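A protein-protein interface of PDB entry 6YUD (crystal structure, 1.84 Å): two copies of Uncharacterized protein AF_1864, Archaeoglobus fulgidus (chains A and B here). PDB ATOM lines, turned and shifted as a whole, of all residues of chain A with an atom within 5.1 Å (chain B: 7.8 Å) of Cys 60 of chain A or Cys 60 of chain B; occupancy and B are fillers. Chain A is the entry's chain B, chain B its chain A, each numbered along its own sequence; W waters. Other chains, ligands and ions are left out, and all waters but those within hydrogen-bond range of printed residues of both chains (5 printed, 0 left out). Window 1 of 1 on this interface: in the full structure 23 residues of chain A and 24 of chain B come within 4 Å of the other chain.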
ATOM      1  N   ILE A  56      21.276   2.867 -31.096  1.00  0.00           N
ATOM      2  CA  ILE A  56      21.989   1.723 -30.466  1.00  0.00           C
ATOM      3  C   ILE A  56      22.565   0.825 -31.565  1.00  0.00           C
ATOM      4  O   ILE A  56      23.718   0.394 -31.399  1.00  0.00           O
ATOM      5  CB  ILE A  56      21.094   0.969 -29.480  1.00  0.00           C
ATOM      6  CG1 ILE A  56      20.557   1.902 -28.394  1.00  0.00           C
ATOM      7  CG2 ILE A  56      21.838  -0.216 -28.885  1.00  0.00           C
ATOM      8  CD1 ILE A  56      19.788   1.212 -27.261  1.00  0.00           C
ATOM      9  N   TRP A  57      21.828   0.602 -32.664  1.00  0.00           N
ATOM     10  CA  TRP A  57      22.304  -0.234 -33.783  1.00  0.00           C
ATOM     11  C   TRP A  57      23.576   0.339 -34.415  1.00  0.00           C
ATOM     12  O   TRP A  57      24.467  -0.439 -34.808  1.00  0.00           O
ATOM     13  CB  TRP A  57      21.202  -0.514 -34.811  1.00  0.00           C
ATOM     14  CG  TRP A  57      20.361   0.623 -35.295  1.00  0.00           C
ATOM     15  CD1 TRP A  57      19.116   0.937 -34.841  1.00  0.00           C
ATOM     16  CD2 TRP A  57      20.592   1.474 -36.435  1.00  0.00           C
ATOM     17  NE1 TRP A  57      18.579   1.953 -35.578  1.00  0.00           N
ATOM     18  CE2 TRP A  57      19.460   2.315 -36.556  1.00  0.00           C
ATOM     19  CE3 TRP A  57      21.651   1.662 -37.325  1.00  0.00           C
ATOM     20  CZ2 TRP A  57      19.368   3.322 -37.520  1.00  0.00           C
ATOM     21  CZ3 TRP A  57      21.540   2.626 -38.303  1.00  0.00           C
ATOM     22  CH2 TRP A  57      20.429   3.457 -38.389  1.00  0.00           C
ATOM     23  N   LEU A  58      23.710   1.656 -34.520  1.00  0.00           N
ATOM     24  CA  LEU A  58      24.955   2.230 -35.066  1.00  0.00           C
ATOM     25  C   LEU A  58      26.127   1.878 -34.145  1.00  0.00           C
ATOM     26  O   LEU A  58      27.199   1.426 -34.654  1.00  0.00           O
ATOM     27  CB  LEU A  58      24.801   3.743 -35.230  1.00  0.00           C
ATOM     28  CG  LEU A  58      26.016   4.458 -35.789  1.00  0.00           C
ATOM     29  CD1 LEU A  58      26.464   3.857 -37.108  1.00  0.00           C
ATOM     30  CD2 LEU A  58      25.671   5.917 -35.996  1.00  0.00           C
ATOM     31  N   HIS A  59      25.962   2.105 -32.855  1.00  0.00           N
ATOM     32  CA  HIS A  59      26.966   1.798 -31.807  1.00  0.00           C
ATOM     33  C   HIS A  59      27.368   0.337 -31.895  1.00  0.00           C
ATOM     34  O   HIS A  59      28.571   0.049 -31.888  1.00  0.00           O
ATOM     35  CB  HIS A  59      26.441   2.141 -30.423  1.00  0.00           C
ATOM     36  CG  HIS A  59      26.654   3.561 -30.031  1.00  0.00           C
ATOM     37  ND1 HIS A  59      27.869   4.013 -29.571  1.00  0.00           N
ATOM     38  CD2 HIS A  59      25.819   4.615 -30.005  1.00  0.00           C
ATOM     39  CE1 HIS A  59      27.777   5.289 -29.307  1.00  0.00           C
ATOM     40  NE2 HIS A  59      26.529   5.681 -29.552  1.00  0.00           N
ATOM     41  N   CYS A  60      26.388  -0.569 -31.992  1.00  0.00           N
ATOM     42  CA  CYS A  60      26.675  -2.011 -32.077  1.00  0.00           C
ATOM     43  C   CYS A  60      27.436  -2.302 -33.365  1.00  0.00           C
ATOM     44  O   CYS A  60      28.405  -3.070 -33.314  1.00  0.00           O
ATOM     45  CB  CYS A  60      25.387  -2.818 -31.928  1.00  0.00           C
ATOM     46  SG  CYS A  60      24.718  -2.745 -30.245  1.00  0.00           S
ATOM     47  N   PHE A  61      27.023  -1.726 -34.487  1.00  0.00           N
ATOM     48  CA  PHE A  61      27.709  -1.907 -35.780  1.00  0.00           C
ATOM     49  C   PHE A  61      29.175  -1.475 -35.646  1.00  0.00           C
ATOM     50  O   PHE A  61      30.097  -2.244 -36.042  1.00  0.00           O
ATOM     51  CB  PHE A  61      26.979  -1.143 -36.875  1.00  0.00           C
ATOM     52  CG  PHE A  61      27.739  -1.060 -38.170  1.00  0.00           C
ATOM     53  CD1 PHE A  61      27.702  -2.100 -39.081  1.00  0.00           C
ATOM     54  CD2 PHE A  61      28.489   0.072 -38.482  1.00  0.00           C
ATOM     55  CE1 PHE A  61      28.408  -2.022 -40.272  1.00  0.00           C
ATOM     56  CE2 PHE A  61      29.178   0.151 -39.682  1.00  0.00           C
ATOM     57  CZ  PHE A  61      29.131  -0.890 -40.576  1.00  0.00           C
ATOM     58  N   LEU A  62      29.413  -0.300 -35.064  1.00  0.00           N
ATOM     59  CA  LEU A  62      30.805   0.189 -34.919  1.00  0.00           C
ATOM     60  C   LEU A  62      31.598  -0.713 -33.967  1.00  0.00           C
ATOM     61  O   LEU A  62      32.751  -1.004 -34.324  1.00  0.00           O
ATOM     62  CB  LEU A  62      30.805   1.673 -34.505  1.00  0.00           C
ATOM     63  CG  LEU A  62      30.200   2.598 -35.559  1.00  0.00           C
ATOM     64  CD1 LEU A  62      29.911   3.973 -34.995  1.00  0.00           C
ATOM     65  CD2 LEU A  62      31.085   2.690 -36.794  1.00  0.00           C
ATOM     66  N   ALA A  63      31.049  -1.128 -32.812  1.00  0.00           N
ATOM     67  CA  ALA A  63      31.771  -1.960 -31.823  1.00  0.00           C
ATOM     68  C   ALA A  63      32.263  -3.257 -32.490  1.00  0.00           C
ATOM     69  O   ALA A  63      33.451  -3.636 -32.303  1.00  0.00           O
ATOM     70  CB  ALA A  63      30.934  -2.231 -30.597  1.00  0.00           C
ATOM     71  N   HIS A  64      31.420  -3.886 -33.319  1.00  0.00           N
ATOM     72  CA  HIS A  64      31.807  -5.093 -34.085  1.00  0.00           C
ATOM     73  C   HIS A  64      32.923  -4.820 -35.107  1.00  0.00           C
ATOM     74  O   HIS A  64      33.814  -5.678 -35.213  1.00  0.00           O
ATOM     75  CB  HIS A  64      30.618  -5.751 -34.777  1.00  0.00           C
ATOM     76  CG  HIS A  64      31.102  -6.979 -35.449  1.00  0.00           C
ATOM     77  ND1 HIS A  64      31.733  -7.992 -34.721  1.00  0.00           N
ATOM     78  CD2 HIS A  64      31.160  -7.317 -36.752  1.00  0.00           C
ATOM     79  CE1 HIS A  64      32.109  -8.928 -35.555  1.00  0.00           C
ATOM     80  NE2 HIS A  64      31.757  -8.542 -36.806  1.00  0.00           N
ATOM     81  N   VAL A  74      32.664   1.668 -24.855  1.00  0.00           N
ATOM     82  CA  VAL A  74      31.522   2.469 -25.332  1.00  0.00           C
ATOM     83  C   VAL A  74      31.351   3.608 -24.339  1.00  0.00           C
ATOM     84  O   VAL A  74      31.262   3.335 -23.144  1.00  0.00           O
ATOM     85  CB  VAL A  74      30.257   1.600 -25.457  1.00  0.00           C
ATOM     86  CG1 VAL A  74      29.062   2.459 -25.820  1.00  0.00           C
ATOM     87  CG2 VAL A  74      30.468   0.535 -26.505  1.00  0.00           C
ATOM     88  N   VAL A  84      33.192  -3.283 -23.354  1.00  0.00           N
ATOM     89  CA  VAL A  84      32.158  -4.275 -23.768  1.00  0.00           C
ATOM     90  C   VAL A  84      32.827  -5.522 -24.367  1.00  0.00           C
ATOM     91  O   VAL A  84      32.146  -6.567 -24.451  1.00  0.00           O
ATOM     92  CB  VAL A  84      31.148  -3.624 -24.723  1.00  0.00           C
ATOM     93  CG1 VAL A  84      30.470  -2.429 -24.063  1.00  0.00           C
ATOM     94  CG2 VAL A  84      31.733  -3.221 -26.082  1.00  0.00           C
ATOM     95  N   GLN A  85      34.086  -5.422 -24.801  1.00  0.00           N
ATOM     96  CA  GLN A  85      34.876  -6.553 -25.377  1.00  0.00           C
ATOM     97  C   GLN A  85      36.337  -6.341 -25.010  1.00  0.00           C
ATOM     98  O   GLN A  85      36.808  -5.212 -25.238  1.00  0.00           O
ATOM     99  CB  GLN A  85      34.845  -6.590 -26.898  1.00  0.00           C
ATOM    100  CG  GLN A  85      33.507  -6.261 -27.508  1.00  0.00           C
ATOM    101  CD  GLN A  85      33.587  -6.304 -29.011  1.00  0.00           C
ATOM    102  OE1 GLN A  85      34.379  -7.079 -29.567  1.00  0.00           O
ATOM    103  NE2 GLN A  85      32.774  -5.469 -29.657  1.00  0.00           N
ATOM    104  N   PHE B  23      15.719  -8.144 -22.798  1.00  0.00           N
ATOM    105  CA  PHE B  23      16.059  -7.922 -21.375  1.00  0.00           C
ATOM    106  C   PHE B  23      15.126  -6.855 -20.791  1.00  0.00           C
ATOM    107  O   PHE B  23      14.573  -6.022 -21.510  1.00  0.00           O
ATOM    108  CB  PHE B  23      17.537  -7.587 -21.191  1.00  0.00           C
ATOM    109  CG  PHE B  23      17.973  -6.286 -21.814  1.00  0.00           C
ATOM    110  CD1 PHE B  23      17.746  -5.087 -21.167  1.00  0.00           C
ATOM    111  CD2 PHE B  23      18.549  -6.263 -23.073  1.00  0.00           C
ATOM    112  CE1 PHE B  23      18.168  -3.894 -21.735  1.00  0.00           C
ATOM    113  CE2 PHE B  23      18.947  -5.070 -23.648  1.00  0.00           C
ATOM    114  CZ  PHE B  23      18.744  -3.887 -22.984  1.00  0.00           C
ATOM    115  N   LEU B  34      28.392  -6.580 -16.107  1.00  0.00           N
ATOM    116  CA  LEU B  34      28.840  -7.343 -17.307  1.00  0.00           C
ATOM    117  C   LEU B  34      29.712  -8.527 -16.849  1.00  0.00           C
ATOM    118  O   LEU B  34      29.697  -9.548 -17.538  1.00  0.00           O
ATOM    119  CB  LEU B  34      29.595  -6.432 -18.281  1.00  0.00           C
ATOM    120  CG  LEU B  34      28.814  -5.226 -18.816  1.00  0.00           C
ATOM    121  CD1 LEU B  34      29.591  -4.563 -19.922  1.00  0.00           C
ATOM    122  CD2 LEU B  34      27.423  -5.612 -19.322  1.00  0.00           C
ATOM    123  N   ILE B  50      18.413  -8.737 -30.446  1.00  0.00           N
ATOM    124  CA  ILE B  50      18.559  -8.272 -29.040  1.00  0.00           C
ATOM    125  C   ILE B  50      17.661  -7.034 -28.856  1.00  0.00           C
ATOM    126  O   ILE B  50      17.679  -6.111 -29.705  1.00  0.00           O
ATOM    127  CB  ILE B  50      20.032  -8.002 -28.719  1.00  0.00           C
ATOM    128  CG1 ILE B  50      20.855  -9.278 -28.922  1.00  0.00           C
ATOM    129  CG2 ILE B  50      20.187  -7.448 -27.313  1.00  0.00           C
ATOM    130  CD1 ILE B  50      22.303  -9.014 -29.165  1.00  0.00           C
ATOM    131  N   PRO B  55      21.382   0.523 -21.294  1.00  0.00           N
ATOM    132  CA  PRO B  55      22.497   1.325 -21.784  1.00  0.00           C
ATOM    133  C   PRO B  55      23.121   0.738 -23.062  1.00  0.00           C
ATOM    134  O   PRO B  55      23.030  -0.483 -23.307  1.00  0.00           O
ATOM    135  CB  PRO B  55      23.455   1.386 -20.597  1.00  0.00           C
ATOM    136  CG  PRO B  55      23.014   0.312 -19.639  1.00  0.00           C
ATOM    137  CD  PRO B  55      21.571  -0.018 -19.951  1.00  0.00           C
ATOM    138  N   ILE B  56      23.675   1.619 -23.891  1.00  0.00           N
ATOM    139  CA  ILE B  56      24.287   1.265 -25.201  1.00  0.00           C
ATOM    140  C   ILE B  56      25.360   0.194 -24.946  1.00  0.00           C
ATOM    141  O   ILE B  56      25.413  -0.761 -25.742  1.00  0.00           O
ATOM    142  CB  ILE B  56      24.820   2.515 -25.909  1.00  0.00           C
ATOM    143  CG1 ILE B  56      23.656   3.463 -26.218  1.00  0.00           C
ATOM    144  CG2 ILE B  56      25.615   2.152 -27.144  1.00  0.00           C
ATOM    145  CD1 ILE B  56      24.000   4.659 -27.035  1.00  0.00           C
ATOM    146  N   TRP B  57      26.106   0.307 -23.840  1.00  0.00           N
ATOM    147  CA  TRP B  57      27.184  -0.652 -23.481  1.00  0.00           C
ATOM    148  C   TRP B  57      26.605  -2.042 -23.177  1.00  0.00           C
ATOM    149  O   TRP B  57      27.312  -3.006 -23.460  1.00  0.00           O
ATOM    150  CB  TRP B  57      28.106  -0.151 -22.363  1.00  0.00           C
ATOM    151  CG  TRP B  57      27.458   0.464 -21.156  1.00  0.00           C
ATOM    152  CD1 TRP B  57      27.266   1.795 -20.922  1.00  0.00           C
ATOM    153  CD2 TRP B  57      27.019  -0.211 -19.963  1.00  0.00           C
ATOM    154  NE1 TRP B  57      26.680   1.981 -19.695  1.00  0.00           N
ATOM    155  CE2 TRP B  57      26.531   0.775 -19.077  1.00  0.00           C
ATOM    156  CE3 TRP B  57      26.949  -1.553 -19.571  1.00  0.00           C
ATOM    157  CZ2 TRP B  57      25.982   0.469 -17.837  1.00  0.00           C
ATOM    158  CZ3 TRP B  57      26.460  -1.848 -18.316  1.00  0.00           C
ATOM    159  CH2 TRP B  57      25.947  -0.857 -17.479  1.00  0.00           C
ATOM    160  N   LEU B  58      25.400  -2.158 -22.622  1.00  0.00           N
ATOM    161  CA  LEU B  58      24.761  -3.488 -22.393  1.00  0.00           C
ATOM    162  C   LEU B  58      24.450  -4.111 -23.752  1.00  0.00           C
ATOM    163  O   LEU B  58      24.730  -5.296 -23.932  1.00  0.00           O
ATOM    164  CB  LEU B  58      23.497  -3.387 -21.534  1.00  0.00           C
ATOM    165  CG  LEU B  58      22.768  -4.700 -21.245  1.00  0.00           C
ATOM    166  CD1 LEU B  58      23.691  -5.730 -20.615  1.00  0.00           C
ATOM    167  CD2 LEU B  58      21.590  -4.427 -20.311  1.00  0.00           C
ATOM    168  N   HIS B  59      23.856  -3.347 -24.648  1.00  0.00           N
ATOM    169  CA  HIS B  59      23.555  -3.780 -26.025  1.00  0.00           C
ATOM    170  C   HIS B  59      24.835  -4.245 -26.737  1.00  0.00           C
ATOM    171  O   HIS B  59      24.805  -5.320 -27.316  1.00  0.00           O
ATOM    172  CB  HIS B  59      22.799  -2.692 -26.762  1.00  0.00           C
ATOM    173  CG  HIS B  59      21.325  -2.731 -26.534  1.00  0.00           C
ATOM    174  ND1 HIS B  59      20.504  -3.556 -27.270  1.00  0.00           N
ATOM    175  CD2 HIS B  59      20.520  -1.993 -25.740  1.00  0.00           C
ATOM    176  CE1 HIS B  59      19.250  -3.358 -26.891  1.00  0.00           C
ATOM    177  NE2 HIS B  59      19.241  -2.406 -25.951  1.00  0.00           N
ATOM    178  N   CYS B  60      25.930  -3.482 -26.661  1.00  0.00           N
ATOM    179  CA  CYS B  60      27.181  -3.794 -27.391  1.00  0.00           C
ATOM    180  C   CYS B  60      27.774  -5.055 -26.768  1.00  0.00           C
ATOM    181  O   CYS B  60      28.266  -5.896 -27.500  1.00  0.00           O
ATOM    182  CB  CYS B  60      28.135  -2.604 -27.352  1.00  0.00           C
ATOM    183  SG  CYS B  60      27.581  -1.205 -28.361  1.00  0.00           S
ATOM    184  N   PHE B  61      27.712  -5.185 -25.449  1.00  0.00           N
ATOM    185  CA  PHE B  61      28.204  -6.367 -24.727  1.00  0.00           C
ATOM    186  C   PHE B  61      27.451  -7.618 -25.235  1.00  0.00           C
ATOM    187  O   PHE B  61      28.098  -8.615 -25.629  1.00  0.00           O
ATOM    188  CB  PHE B  61      28.085  -6.128 -23.229  1.00  0.00           C
ATOM    189  CG  PHE B  61      28.406  -7.352 -22.421  1.00  0.00           C
ATOM    190  CD1 PHE B  61      29.713  -7.707 -22.156  1.00  0.00           C
ATOM    191  CD2 PHE B  61      27.394  -8.229 -22.045  1.00  0.00           C
ATOM    192  CE1 PHE B  61      29.997  -8.865 -21.431  1.00  0.00           C
ATOM    193  CE2 PHE B  61      27.678  -9.380 -21.318  1.00  0.00           C
ATOM    194  CZ  PHE B  61      28.980  -9.721 -21.058  1.00  0.00           C
ATOM    195  N   LEU B  62      26.128  -7.554 -25.283  1.00  0.00           N
ATOM    196  CA  LEU B  62      25.276  -8.714 -25.661  1.00  0.00           C
ATOM    197  C   LEU B  62      25.488  -9.051 -27.126  1.00  0.00           C
ATOM    198  O   LEU B  62      25.698 -10.245 -27.405  1.00  0.00           O
ATOM    199  CB  LEU B  62      23.810  -8.387 -25.376  1.00  0.00           C
ATOM    200  CG  LEU B  62      23.458  -8.269 -23.904  1.00  0.00           C
ATOM    201  CD1 LEU B  62      22.040  -7.767 -23.734  1.00  0.00           C
ATOM    202  CD2 LEU B  62      23.675  -9.582 -23.177  1.00  0.00           C
ATOM    203  N   ALA B  63      25.568  -8.038 -28.005  1.00  0.00           N
ATOM    204  CA  ALA B  63      25.733  -8.237 -29.454  1.00  0.00           C
ATOM    205  C   ALA B  63      27.036  -9.010 -29.691  1.00  0.00           C
ATOM    206  O   ALA B  63      27.050  -9.941 -30.544  1.00  0.00           O
ATOM    207  CB  ALA B  63      25.695  -6.912 -30.184  1.00  0.00           C
ATOM    208  N   HIS B  64      28.093  -8.651 -28.972  1.00  0.00           N
ATOM    209  CA  HIS B  64      29.394  -9.350 -29.082  1.00  0.00           C
ATOM    210  C   HIS B  64      29.246 -10.805 -28.610  1.00  0.00           C
ATOM    211  O   HIS B  64      29.980 -11.660 -29.123  1.00  0.00           O
ATOM    212  CB  HIS B  64      30.492  -8.658 -28.263  1.00  0.00           C
ATOM    213  CG  HIS B  64      31.753  -9.434 -28.340  1.00  0.00           C
ATOM    214  ND1 HIS B  64      32.374  -9.680 -29.580  1.00  0.00           N
ATOM    215  CD2 HIS B  64      32.443 -10.114 -27.406  1.00  0.00           C
ATOM    216  CE1 HIS B  64      33.426 -10.441 -29.383  1.00  0.00           C
ATOM    217  NE2 HIS B  64      33.493 -10.725 -28.055  1.00  0.00           N
ATOM    218  N   LYS B  65      28.389 -11.066 -27.628  1.00  0.00           N
ATOM    219  CA  LYS B  65      28.263 -12.410 -27.002  1.00  0.00           C
ATOM    220  C   LYS B  65      27.507 -13.342 -27.955  1.00  0.00           C
ATOM    221  O   LYS B  65      27.566 -14.552 -27.727  1.00  0.00           O
ATOM    222  CB  LYS B  65      27.592 -12.328 -25.622  1.00  0.00           C
ATOM    223  CG  LYS B  65      28.488 -11.773 -24.526  1.00  0.00           C
ATOM    224  CD  LYS B  65      29.565 -12.751 -24.091  1.00  0.00           C
ATOM    225  CE  LYS B  65      30.505 -12.212 -23.032  1.00  0.00           C
ATOM    226  NZ  LYS B  65      31.639 -11.474 -23.646  1.00  0.00           N
ATOM    227  N   TYR B  66      26.863 -12.831 -29.011  1.00  0.00           N
ATOM    228  CA  TYR B  66      26.179 -13.697 -30.018  1.00  0.00           C
ATOM    229  C   TYR B  66      26.846 -13.621 -31.396  1.00  0.00           C
ATOM    230  O   TYR B  66      26.232 -14.045 -32.406  1.00  0.00           O
ATOM    231  CB  TYR B  66      24.693 -13.355 -30.020  1.00  0.00           C
ATOM    232  CG  TYR B  66      24.066 -13.681 -28.702  1.00  0.00           C
ATOM    233  CD1 TYR B  66      23.817 -15.006 -28.343  1.00  0.00           C
ATOM    234  CD2 TYR B  66      23.754 -12.686 -27.794  1.00  0.00           C
ATOM    235  CE1 TYR B  66      23.262 -15.325 -27.116  1.00  0.00           C
ATOM    236  CE2 TYR B  66      23.170 -12.992 -26.576  1.00  0.00           C
ATOM    237  CZ  TYR B  66      22.924 -14.318 -26.234  1.00  0.00           C
ATOM    238  OH  TYR B  66      22.385 -14.614 -25.009  1.00  0.00           O
ATOM    239  N   VAL B  72      23.597 -10.889 -35.961  1.00  0.00           N
ATOM    240  CA  VAL B  72      23.043 -10.211 -34.775  1.00  0.00           C
ATOM    241  C   VAL B  72      22.300  -8.976 -35.284  1.00  0.00           C
ATOM    242  O   VAL B  72      22.858  -8.204 -36.093  1.00  0.00           O
ATOM    243  CB  VAL B  72      24.125  -9.863 -33.746  1.00  0.00           C
ATOM    244  CG1 VAL B  72      23.518  -9.134 -32.557  1.00  0.00           C
ATOM    245  CG2 VAL B  72      24.906 -11.098 -33.307  1.00  0.00           C
ATOM    246  N   ALA B  73      21.092  -8.784 -34.769  1.00  0.00           N
ATOM    247  CA  ALA B  73      20.230  -7.643 -35.108  1.00  0.00           C
ATOM    248  C   ALA B  73      19.824  -6.986 -33.802  1.00  0.00           C
ATOM    249  O   ALA B  73      19.711  -7.679 -32.797  1.00  0.00           O
ATOM    250  CB  ALA B  73      19.065  -8.085 -35.957  1.00  0.00           C
ATOM    251  N   VAL B  74      19.799  -5.658 -33.803  1.00  0.00           N
ATOM    252  CA  VAL B  74      19.465  -4.843 -32.613  1.00  0.00           C
ATOM    253  C   VAL B  74      18.086  -4.234 -32.831  1.00  0.00           C
ATOM    254  O   VAL B  74      17.850  -3.634 -33.910  1.00  0.00           O
ATOM    255  CB  VAL B  74      20.533  -3.769 -32.366  1.00  0.00           C
ATOM    256  CG1 VAL B  74      20.119  -2.903 -31.206  1.00  0.00           C
ATOM    257  CG2 VAL B  74      21.888  -4.406 -32.125  1.00  0.00           C
ATOM    258  N   VAL B  82      17.536  -4.079 -36.701  1.00  0.00           N
ATOM    259  CA  VAL B  82      18.616  -3.689 -37.629  1.00  0.00           C
ATOM    260  C   VAL B  82      19.742  -4.704 -37.523  1.00  0.00           C
ATOM    261  O   VAL B  82      20.279  -4.890 -36.420  1.00  0.00           O
ATOM    262  CB  VAL B  82      19.115  -2.260 -37.320  1.00  0.00           C
ATOM    263  CG1 VAL B  82      20.177  -1.860 -38.298  1.00  0.00           C
ATOM    264  CG2 VAL B  82      17.960  -1.272 -37.359  1.00  0.00           C
ATOM    265  N   VAL B  83      20.125  -5.286 -38.649  1.00  0.00           N
ATOM    266  CA  VAL B  83      21.274  -6.234 -38.679  1.00  0.00           C
ATOM    267  C   VAL B  83      22.567  -5.422 -38.483  1.00  0.00           C
ATOM    268  O   VAL B  83      22.870  -4.566 -39.316  1.00  0.00           O
ATOM    269  CB  VAL B  83      21.292  -7.072 -39.959  1.00  0.00           C
ATOM    270  CG1 VAL B  83      22.535  -7.940 -40.007  1.00  0.00           C
ATOM    271  CG2 VAL B  83      20.028  -7.935 -40.100  1.00  0.00           C
ATOM    272  N   VAL B  84      23.300  -5.682 -37.409  1.00  0.00           N
ATOM    273  CA  VAL B  84      24.564  -4.946 -37.110  1.00  0.00           C
ATOM    274  C   VAL B  84      25.780  -5.845 -37.367  1.00  0.00           C
ATOM    275  O   VAL B  84      26.900  -5.315 -37.476  1.00  0.00           O
ATOM    276  CB  VAL B  84      24.535  -4.431 -35.670  1.00  0.00           C
ATOM    277  CG1 VAL B  84      23.357  -3.481 -35.475  1.00  0.00           C
ATOM    278  CG2 VAL B  84      24.487  -5.576 -34.669  1.00  0.00           C
ATOM    279  N   GLN B  85      25.586  -7.159 -37.413  1.00  0.00           N
ATOM    280  CA  GLN B  85      26.649  -8.149 -37.728  1.00  0.00           C
ATOM    281  C   GLN B  85      26.022  -9.215 -38.619  1.00  0.00           C
ATOM    282  O   GLN B  85      24.948  -9.736 -38.266  1.00  0.00           O
ATOM    283  CB  GLN B  85      27.163  -8.893 -36.496  1.00  0.00           C
ATOM    284  CG  GLN B  85      27.710  -8.033 -35.381  1.00  0.00           C
ATOM    285  CD  GLN B  85      27.968  -8.826 -34.128  1.00  0.00           C
ATOM    286  OE1 GLN B  85      28.373  -9.989 -34.171  1.00  0.00           O
ATOM    287  NE2 GLN B  85      27.797  -8.168 -32.998  1.00  0.00           N
HETATM  288  O   HOH W   1      28.185  -5.608 -32.038  1.00  0.00           O
HETATM  289  O   HOH W   2      31.812  -8.553 -31.773  1.00  0.00           O
HETATM  290  O   HOH W   3      29.658  -5.251 -29.919  1.00  0.00           O
HETATM  291  O   HOH W   4      29.619  -4.615 -37.638  1.00  0.00           O
HETATM  292  O   HOH W   5      30.864  -8.848 -25.063  1.00  0.00           O
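Leu 58 of chain A touches none of the printed residues of chain B.
Of the printed residues of chain B, Cys 60 of chain A touches His 59, Cys 60, Val 74 and Val 84.
Of the printed residues of chain B, His 64 of chain A touches Gln 85 (3.6 Å).
Printed residues of chain B within 4 Å of Val 84 of chain A: Trp 57 (3.3 Å), Cys 60 (3.9 Å) and Phe 61 (3.5 Å).
Cys 60 of chain B touches just these residues of chain A: His 59 (3.9 Å), Cys 60 (3.8 Å), Val 74 (3.8 Å) and Val 84 (3.9 Å).
Printed residues of chain A within 4 Å of Val 82 of chain B: Trp 57 (3.5 Å).
Printed residues of chain A within 4 Å of Gln 85 of chain B: His 64.
The nearest residue of chain A that does not touch Cys 60 of chain B is Ala 63 of chain A (4.2 Å).
The nearest printed residue of chain A that does not touch His 64 of chain B is Val 84 of chain A (4.6 Å).
Water W2 bridges ND1 of His 64 of chain B (2.5 Å) and ND1 of His 64 of chain A (3.0 Å).
Water W5 lies within hydrogen-bond range of O of Val 84 of chain A (2.7 Å), O of Phe 61 of chain B (2.8 Å) and NZ of Lys 65 of chain B (3.1 Å).
Water W1 bridges NE2 of Gln 85 of chain B (2.8 Å) and O of Cys 60 of chain A (2.8 Å).
Water W4 bridges O of Val 84 of chain B and O of Phe 61 of chain A.
Water W3 lies within hydrogen-bond range of the backbone carbonyl oxygen of Cys 60 of chain B (2.9 Å) and the side-chain amide nitrogen of Gln 85 of chain A (3.1 Å).
Ile 56 of chain A touches Val 74 of chain B, and with the chains exchanged Val 74 of chain A touches Ile 56 of chain B.
Trp 57 of chain A touches Val 84 of chain B, and with the chains exchanged Val 84 of chain A touches Trp 57 of chain B.
Cys 60 of chain A touches its own counterpart, Cys 60 of chain B.
Cys 60 of chain A touches Val 74 of chain B, and with the chains exchanged Val 74 of chain A touches Cys 60 of chain B.
Positions printed for both chains: 56, 57, 58, 59, 60, 61, 62, 63, 64, 74, 84 and 85.
Of the 18 pairs that touch across the chains among the printed residues, 17 have their exchanged pair printed and touching as well.
SG of Cys 60 of chain B lies within hydrogen-bond range of SG of Cys 60 of chain A.
OE1 of Gln 85 of chain A is in hydrogen-bond range of ND1 of His 64 of chain B (3.3 Å).
The backbone carbonyl oxygen (O) of Ile 56 of chain B lies within hydrogen-bond range of the side-chain sulfur (SG) of Cys 60 of chain B, at 3.4 Å.
The backbone carbonyl oxygen of Ala 63 of chain B lies within hydrogen-bond range of the side-chain amide nitrogen of Gln 85 of chain B (3.1 Å).
N of Val 84 of chain B sits at hydrogen-bond distance from O of Val 72 of chain B, at 2.9 Å.
The backbone carbonyl oxygen (O) of Gln 85 of chain B sits at hydrogen-bond distance from the backbone NH (N) of Val 72 of chain B (2.9 Å).
The backbone carbonyl oxygen (O) of Ile 56 of chain A is in hydrogen-bond range of the side-chain sulfur (SG) of Cys 60 of chain A.
O of Ala 63 of chain A lies within hydrogen-bond range of NE2 of Gln 85 of chain A (3.3 Å).
Among the printed residues, pairs that only touch across the chains: Val 84 of chain A with Trp 57 of chain B (3.3 Å), Trp 57 of chain A with Val 84 of chain B (3.3 Å), His 59 of chain A with Ile 56 of chain B (3.4 Å), Ile 56 of chain A with His 59 of chain B (3.4 Å), Val 84 of chain A with Phe 61 of chain B (3.5 Å), Trp 57 of chain A with Val 82 of chain B (3.5 Å), His 64 of chain A with Gln 85 of chain B (3.6 Å), Phe 61 of chain A with Val 84 of chain B (3.7 Å), Val 74 of chain A with Ile 56 of chain B (3.7 Å), Cys 60 of chain A with Val 74 of chain B (3.8 Å), Cys 60 of chain A with His 59 of chain B (3.8 Å), Val 74 of chain A with Cys 60 of chain B (3.8 Å), His 59 of chain A with Cys 60 of chain B (3.9 Å), Val 84 of chain A with Cys 60 of chain B (3.9 Å), Ile 56 of chain A with Val 74 of chain B (3.9 Å) and Cys 60 of chain A with Val 84 of chain B (3.99 Å).
Hydrophobic or aromatic side chains of chain B within 4 Å of the printed part of chain A: Ile 56, Trp 57, His 59, Phe 61, His 64, Val 74, Val 82 and Val 84.
Hydrophobic or aromatic side chains of chain A within 4 Å of the printed part of chain B: Ile 56, Trp 57, His 59, Phe 61, His 64, Val 74 and Val 84.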
